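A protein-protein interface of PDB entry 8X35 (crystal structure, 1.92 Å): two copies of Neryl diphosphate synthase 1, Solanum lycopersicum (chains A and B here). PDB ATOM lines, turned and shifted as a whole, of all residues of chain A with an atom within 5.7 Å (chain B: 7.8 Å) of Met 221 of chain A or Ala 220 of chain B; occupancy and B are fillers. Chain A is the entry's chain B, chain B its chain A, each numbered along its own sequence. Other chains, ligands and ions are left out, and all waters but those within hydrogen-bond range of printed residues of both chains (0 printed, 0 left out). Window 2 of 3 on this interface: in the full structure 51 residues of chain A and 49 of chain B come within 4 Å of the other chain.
SD of Met 221 of chain A sits close to O of Ala 220 of chain B (3.5 Å).
The backbone carbonyl oxygen (O) of Asn 218 of chain A is in hydrogen-bond range of the side-chain amide nitrogen (ND2) of Asn 222 of chain A.
Val 217 of chain A touches Val 217 of chain B (CG2 to CG2, 3.7 Å). CG1 of Val 217 of chain A touches CB of Ala 220 of chain B, 3.9 Å away. Val 227 of chain B touches Val 217 of chain A. CG2 of Val 217 of chain A touches CD1 of Ile 230 of chain B (3.9 Å). Asn 218 of chain A touches Val 227 of chain B. CB of Ala 220 of chain A touches CG1 of Val 217 of chain B, at 3.7 Å. Met 221 of chain A touches Met 221 of chain B.
Of chain B, only Ala 220 (3.5 Å) and Met 221 (3.97 Å) come within 4 Å of Met 221 of chain A. Ala 220 of chain A touches just one residue of chain B: Val 217. Of the printed residues of chain A, Ile 230 of chain B touches Val 217 (3.9 Å). Printed residues of chain B within 4 Å of Asn 218 of chain A: Val 227 (3.4 Å). Of the printed residues of chain A, Met 221 of chain B touches Met 221. The nearest residue of chain B that does not touch Met 221 of chain A is Leu 225 of chain B (4.9 Å). The nearest printed residue of chain A that does not touch Val 227 of chain B is Met 221 of chain A (5.6 Å).
Printed residues of chain B that touch a printed residue of chain A: Val 217, Ala 220, Met 221, Val 227 and Ile 230. Hydrophobic or aromatic side chains of chain B that line the printed part of chain A: Val 217, Ala 220, Val 227 and Ile 230. Hydrophobic or aromatic side chains of chain A that line the printed part of chain B: Val 217, Ala 220 and Met 221. Among the printed residues, 8 pairs touch across the chains.
Val 217 of chain B touches its own counterpart, Val 217 of chain A. Val 217 of chain A touches Ala 220 of chain B, and with the chains exchanged Ala 220 of chain A touches Val 217 of chain B. Met 221 of chain A touches Ala 220 of chain B, but with the chains exchanged Ala 220 of chain A does not touch Met 221 of chain B (4.04 Å). Met 221 of chain A touches its own counterpart, Met 221 of chain B. Positions printed for both chains: 216, 217, 218, 219, 220, 221, 222 and 223. Of the 8 pairs that touch across the chains among the printed residues, 4 have their exchanged pair printed and touching as well.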
ATOM      1  N   ILE A 216       8.709  15.034  -1.051  1.00  0.00           N
ATOM      2  CA  ILE A 216       9.843  14.134  -1.295  1.00  0.00           C
ATOM      3  C   ILE A 216       9.591  13.233  -2.508  1.00  0.00           C
ATOM      4  O   ILE A 216      10.501  12.986  -3.312  1.00  0.00           O
ATOM      5  CB  ILE A 216      10.143  13.317  -0.018  1.00  0.00           C
ATOM      6  CG1 ILE A 216      10.660  14.238   1.086  1.00  0.00           C
ATOM      7  CG2 ILE A 216      11.138  12.210  -0.278  1.00  0.00           C
ATOM      8  CD1 ILE A 216      10.910  13.501   2.428  1.00  0.00           C
ATOM      9  N   VAL A 217       8.369  12.715  -2.663  1.00  0.00           N
ATOM     10  CA  VAL A 217       8.047  11.902  -3.837  1.00  0.00           C
ATOM     11  C   VAL A 217       8.212  12.710  -5.128  1.00  0.00           C
ATOM     12  O   VAL A 217       8.764  12.217  -6.126  1.00  0.00           O
ATOM     13  CB  VAL A 217       6.624  11.330  -3.716  1.00  0.00           C
ATOM     14  CG1 VAL A 217       6.135  10.812  -5.059  1.00  0.00           C
ATOM     15  CG2 VAL A 217       6.579  10.208  -2.645  1.00  0.00           C
ATOM     16  N   ASN A 218       7.720  13.952  -5.138  1.00  0.00           N
ATOM     17  CA  ASN A 218       7.763  14.758  -6.356  1.00  0.00           C
ATOM     18  C   ASN A 218       9.197  15.079  -6.757  1.00  0.00           C
ATOM     19  O   ASN A 218       9.511  15.170  -7.951  1.00  0.00           O
ATOM     20  CB  ASN A 218       6.978  16.056  -6.162  1.00  0.00           C
ATOM     21  CG  ASN A 218       5.549  15.929  -6.633  1.00  0.00           C
ATOM     22  OD1 ASN A 218       5.266  15.257  -7.632  1.00  0.00           O
ATOM     23  ND2 ASN A 218       4.626  16.569  -5.908  1.00  0.00           N
ATOM     24  N   LYS A 219      10.074  15.280  -5.770  1.00  0.00           N
ATOM     25  CA  LYS A 219      11.491  15.464  -6.060  1.00  0.00           C
ATOM     26  C   LYS A 219      12.122  14.187  -6.621  1.00  0.00           C
ATOM     27  O   LYS A 219      12.843  14.241  -7.620  1.00  0.00           O
ATOM     28  CB  LYS A 219      12.217  15.942  -4.806  1.00  0.00           C
ATOM     29  CG  LYS A 219      11.856  17.369  -4.417  1.00  0.00           C
ATOM     30  CD  LYS A 219      12.748  17.872  -3.283  1.00  0.00           C
ATOM     31  CE  LYS A 219      12.018  18.816  -2.367  1.00  0.00           C
ATOM     32  NZ  LYS A 219      11.870  20.178  -2.883  1.00  0.00           N
ATOM     33  N   ALA A 220      11.874  13.022  -5.996  1.00  0.00           N
ATOM     34  CA  ALA A 220      12.432  11.770  -6.518  1.00  0.00           C
ATOM     35  C   ALA A 220      11.962  11.488  -7.943  1.00  0.00           C
ATOM     36  O   ALA A 220      12.717  10.957  -8.770  1.00  0.00           O
ATOM     37  CB  ALA A 220      12.048  10.600  -5.611  1.00  0.00           C
ATOM     38  N   MET A 221      10.702  11.794  -8.236  1.00  0.00           N
ATOM     39  CA  MET A 221      10.139  11.554  -9.557  1.00  0.00           C
ATOM     40  C   MET A 221      10.759  12.461 -10.620  1.00  0.00           C
ATOM     41  O   MET A 221      10.714  12.133 -11.812  1.00  0.00           O
ATOM     42  CB  MET A 221       8.635  11.793  -9.500  1.00  0.00           C
ATOM     43  CG  MET A 221       7.868  10.717  -8.755  1.00  0.00           C
ATOM     44  SD  MET A 221       7.454   9.282  -9.714  1.00  0.00           S
ATOM     45  CE  MET A 221       5.778   9.776 -10.163  1.00  0.00           C
ATOM     46  N   ASN A 222      11.315  13.598 -10.214  1.00  0.00           N
ATOM     47  CA  ASN A 222      11.949  14.553 -11.116  1.00  0.00           C
ATOM     48  C   ASN A 222      13.470  14.517 -11.038  1.00  0.00           C
ATOM     49  O   ASN A 222      14.125  15.481 -11.458  1.00  0.00           O
ATOM     50  CB  ASN A 222      11.462  15.973 -10.821  1.00  0.00           C
ATOM     51  CG  ASN A 222      10.002  16.161 -11.130  1.00  0.00           C
ATOM     52  OD1 ASN A 222       9.491  15.625 -12.110  1.00  0.00           O
ATOM     53  ND2 ASN A 222       9.310  16.920 -10.285  1.00  0.00           N
ATOM     54  N   GLY A 223      14.041  13.450 -10.483  1.00  0.00           N
ATOM     55  CA  GLY A 223      15.480  13.253 -10.470  1.00  0.00           C
ATOM     56  C   GLY A 223      16.262  14.159  -9.550  1.00  0.00           C
ATOM     57  O   GLY A 223      17.495  14.174  -9.628  1.00  0.00           O
ATOM     58  N   THR B 213       8.238   5.932   4.006  1.00  0.00           N
ATOM     59  CA  THR B 213       8.416   6.935   2.945  1.00  0.00           C
ATOM     60  C   THR B 213       9.195   6.363   1.755  1.00  0.00           C
ATOM     61  O   THR B 213       8.800   6.542   0.597  1.00  0.00           O
ATOM     62  CB  THR B 213       9.119   8.165   3.512  1.00  0.00           C
ATOM     63  OG1 THR B 213       8.311   8.744   4.545  1.00  0.00           O
ATOM     64  CG2 THR B 213       9.323   9.244   2.409  1.00  0.00           C
ATOM     65  N   LYS B 214      10.314   5.687   2.024  1.00  0.00           N
ATOM     66  CA  LYS B 214      11.089   5.047   0.954  1.00  0.00           C
ATOM     67  C   LYS B 214      10.259   4.028   0.175  1.00  0.00           C
ATOM     68  O   LYS B 214      10.418   3.890  -1.048  1.00  0.00           O
ATOM     69  CB  LYS B 214      12.318   4.348   1.541  1.00  0.00           C
ATOM     70  CG  LYS B 214      13.341   5.268   2.169  1.00  0.00           C
ATOM     71  CD  LYS B 214      14.481   4.407   2.664  1.00  0.00           C
ATOM     72  CE  LYS B 214      15.530   5.241   3.338  1.00  0.00           C
ATOM     73  NZ  LYS B 214      16.418   4.343   4.136  1.00  0.00           N
ATOM     74  N   SER B 215       9.399   3.268   0.868  1.00  0.00           N
ATOM     75  CA  SER B 215       8.544   2.320   0.167  1.00  0.00           C
ATOM     76  C   SER B 215       7.559   3.035  -0.762  1.00  0.00           C
ATOM     77  O   SER B 215       7.347   2.602  -1.905  1.00  0.00           O
ATOM     78  CB  SER B 215       7.809   1.428   1.170  1.00  0.00           C
ATOM     79  OG  SER B 215       6.980   0.492   0.497  1.00  0.00           O
ATOM     80  N   ILE B 216       6.956   4.135  -0.296  1.00  0.00           N
ATOM     81  CA  ILE B 216       6.028   4.887  -1.133  1.00  0.00           C
ATOM     82  C   ILE B 216       6.755   5.519  -2.321  1.00  0.00           C
ATOM     83  O   ILE B 216       6.216   5.582  -3.433  1.00  0.00           O
ATOM     84  CB  ILE B 216       5.298   5.946  -0.283  1.00  0.00           C
ATOM     85  CG1 ILE B 216       4.374   5.272   0.739  1.00  0.00           C
ATOM     86  CG2 ILE B 216       4.533   6.937  -1.164  1.00  0.00           C
ATOM     87  CD1 ILE B 216       3.872   6.262   1.791  1.00  0.00           C
ATOM     88  N   VAL B 217       7.981   6.001  -2.108  1.00  0.00           N
ATOM     89  CA  VAL B 217       8.753   6.583  -3.206  1.00  0.00           C
ATOM     90  C   VAL B 217       9.037   5.531  -4.284  1.00  0.00           C
ATOM     91  O   VAL B 217       8.962   5.814  -5.485  1.00  0.00           O
ATOM     92  CB  VAL B 217      10.055   7.214  -2.670  1.00  0.00           C
ATOM     93  CG1 VAL B 217      11.008   7.551  -3.826  1.00  0.00           C
ATOM     94  CG2 VAL B 217       9.747   8.474  -1.859  1.00  0.00           C
ATOM     95  N   ASN B 218       9.347   4.295  -3.874  1.00  0.00           N
ATOM     96  CA  ASN B 218       9.647   3.254  -4.858  1.00  0.00           C
ATOM     97  C   ASN B 218       8.406   2.853  -5.641  1.00  0.00           C
ATOM     98  O   ASN B 218       8.491   2.545  -6.838  1.00  0.00           O
ATOM     99  CB  ASN B 218      10.270   2.044  -4.176  1.00  0.00           C
ATOM    100  CG  ASN B 218      11.769   2.170  -4.047  1.00  0.00           C
ATOM    101  OD1 ASN B 218      12.459   2.532  -5.008  1.00  0.00           O
ATOM    102  ND2 ASN B 218      12.287   1.890  -2.859  1.00  0.00           N
ATOM    103  N   LYS B 219       7.241   2.853  -4.989  1.00  0.00           N
ATOM    104  CA  LYS B 219       6.003   2.566  -5.707  1.00  0.00           C
ATOM    105  C   LYS B 219       5.705   3.640  -6.747  1.00  0.00           C
ATOM    106  O   LYS B 219       5.252   3.325  -7.855  1.00  0.00           O
ATOM    107  CB  LYS B 219       4.840   2.425  -4.727  1.00  0.00           C
ATOM    108  CG  LYS B 219       4.877   1.116  -3.910  1.00  0.00           C
ATOM    109  CD  LYS B 219       3.596   0.934  -3.114  1.00  0.00           C
ATOM    110  CE  LYS B 219       3.599  -0.371  -2.317  1.00  0.00           C
ATOM    111  NZ  LYS B 219       4.842  -0.521  -1.508  1.00  0.00           N
ATOM    112  N   ALA B 220       5.937   4.913  -6.409  1.00  0.00           N
ATOM    113  CA  ALA B 220       5.689   5.973  -7.384  1.00  0.00           C
ATOM    114  C   ALA B 220       6.627   5.846  -8.581  1.00  0.00           C
ATOM    115  O   ALA B 220       6.200   5.976  -9.735  1.00  0.00           O
ATOM    116  CB  ALA B 220       5.840   7.351  -6.733  1.00  0.00           C
ATOM    117  N   MET B 221       7.911   5.591  -8.322  1.00  0.00           N
ATOM    118  CA  MET B 221       8.893   5.478  -9.386  1.00  0.00           C
ATOM    119  C   MET B 221       8.671   4.245 -10.245  1.00  0.00           C
ATOM    120  O   MET B 221       9.209   4.177 -11.353  1.00  0.00           O
ATOM    121  CB  MET B 221      10.305   5.473  -8.794  1.00  0.00           C
ATOM    122  CG  MET B 221      10.722   6.882  -8.374  1.00  0.00           C
ATOM    123  SD  MET B 221      12.372   7.085  -7.667  1.00  0.00           S
ATOM    124  CE  MET B 221      12.736   5.432  -7.100  1.00  0.00           C
ATOM    125  N   ASN B 222       7.878   3.286  -9.780  1.00  0.00           N
ATOM    126  CA  ASN B 222       7.500   2.140 -10.584  1.00  0.00           C
ATOM    127  C   ASN B 222       6.111   2.280 -11.191  1.00  0.00           C
ATOM    128  O   ASN B 222       5.575   1.301 -11.716  1.00  0.00           O
ATOM    129  CB  ASN B 222       7.580   0.869  -9.750  1.00  0.00           C
ATOM    130  CG  ASN B 222       8.957   0.252  -9.786  1.00  0.00           C
ATOM    131  OD1 ASN B 222       9.898   0.777  -9.178  1.00  0.00           O
ATOM    132  ND2 ASN B 222       9.093  -0.861 -10.509  1.00  0.00           N
ATOM    133  N   GLY B 223       5.518   3.469 -11.136  1.00  0.00           N
ATOM    134  CA  GLY B 223       4.234   3.691 -11.775  1.00  0.00           C
ATOM    135  C   GLY B 223       3.037   3.091 -11.072  1.00  0.00           C
ATOM    136  O   GLY B 223       2.000   2.885 -11.711  1.00  0.00           O
ATOM    137  N   LEU B 224       3.134   2.833  -9.766  1.00  0.00           N
ATOM    138  CA  LEU B 224       2.070   2.170  -9.017  1.00  0.00           C
ATOM    139  C   LEU B 224       1.136   3.131  -8.289  1.00  0.00           C
ATOM    140  O   LEU B 224       0.060   2.708  -7.852  1.00  0.00           O
ATOM    141  CB  LEU B 224       2.668   1.185  -8.003  1.00  0.00           C
ATOM    142  CG  LEU B 224       2.928  -0.222  -8.544  1.00  0.00           C
ATOM    143  CD1 LEU B 224       4.234  -0.254  -9.306  1.00  0.00           C
ATOM    144  CD2 LEU B 224       2.925  -1.258  -7.426  1.00  0.00           C
ATOM    145  N   LEU B 225       1.507   4.402  -8.145  1.00  0.00           N
ATOM    146  CA  LEU B 225       0.625   5.358  -7.494  1.00  0.00           C
ATOM    147  C   LEU B 225       1.051   6.766  -7.866  1.00  0.00           C
ATOM    148  O   LEU B 225       2.206   7.014  -8.222  1.00  0.00           O
ATOM    149  CB  LEU B 225       0.640   5.206  -5.970  1.00  0.00           C
ATOM    150  CG  LEU B 225       2.003   5.083  -5.298  1.00  0.00           C
ATOM    151  CD1 LEU B 225       2.520   6.459  -4.910  1.00  0.00           C
ATOM    152  CD2 LEU B 225       1.838   4.258  -4.054  1.00  0.00           C
ATOM    153  N   ASP B 226       0.112   7.692  -7.721  1.00  0.00           N
ATOM    154  CA  ASP B 226       0.338   9.104  -7.976  1.00  0.00           C
ATOM    155  C   ASP B 226       0.404   9.862  -6.652  1.00  0.00           C
ATOM    156  O   ASP B 226      -0.149   9.427  -5.641  1.00  0.00           O
ATOM    157  CB  ASP B 226      -0.784   9.674  -8.851  1.00  0.00           C
ATOM    158  CG  ASP B 226      -0.882   8.993 -10.208  1.00  0.00           C
ATOM    159  OD1 ASP B 226       0.170   8.746 -10.840  1.00  0.00           O
ATOM    160  OD2 ASP B 226      -2.021   8.673 -10.623  1.00  0.00           O
ATOM    161  N   VAL B 227       1.074  11.019  -6.670  1.00  0.00           N
ATOM    162  CA  VAL B 227       1.189  11.838  -5.463  1.00  0.00           C
ATOM    163  C   VAL B 227      -0.182  12.106  -4.846  1.00  0.00           C
ATOM    164  O   VAL B 227      -0.321  12.169  -3.616  1.00  0.00           O
ATOM    165  CB  VAL B 227       1.934  13.156  -5.787  1.00  0.00           C
ATOM    166  CG1 VAL B 227       1.832  14.132  -4.637  1.00  0.00           C
ATOM    167  CG2 VAL B 227       3.390  12.878  -6.107  1.00  0.00           C
ATOM    168  N   ILE B 230      -1.535   9.719  -2.013  1.00  0.00           N
ATOM    169  CA  ILE B 230      -0.867   9.603  -0.717  1.00  0.00           C
ATOM    170  C   ILE B 230      -1.792  10.158   0.364  1.00  0.00           C
ATOM    171  O   ILE B 230      -2.098  11.352   0.390  1.00  0.00           O
ATOM    172  CB  ILE B 230       0.496  10.306  -0.727  1.00  0.00           C
ATOM    173  CG1 ILE B 230       1.394   9.678  -1.804  1.00  0.00           C
ATOM    174  CG2 ILE B 230       1.167  10.237   0.636  1.00  0.00           C
ATOM    175  CD1 ILE B 230       2.719  10.413  -2.048  1.00  0.00           C
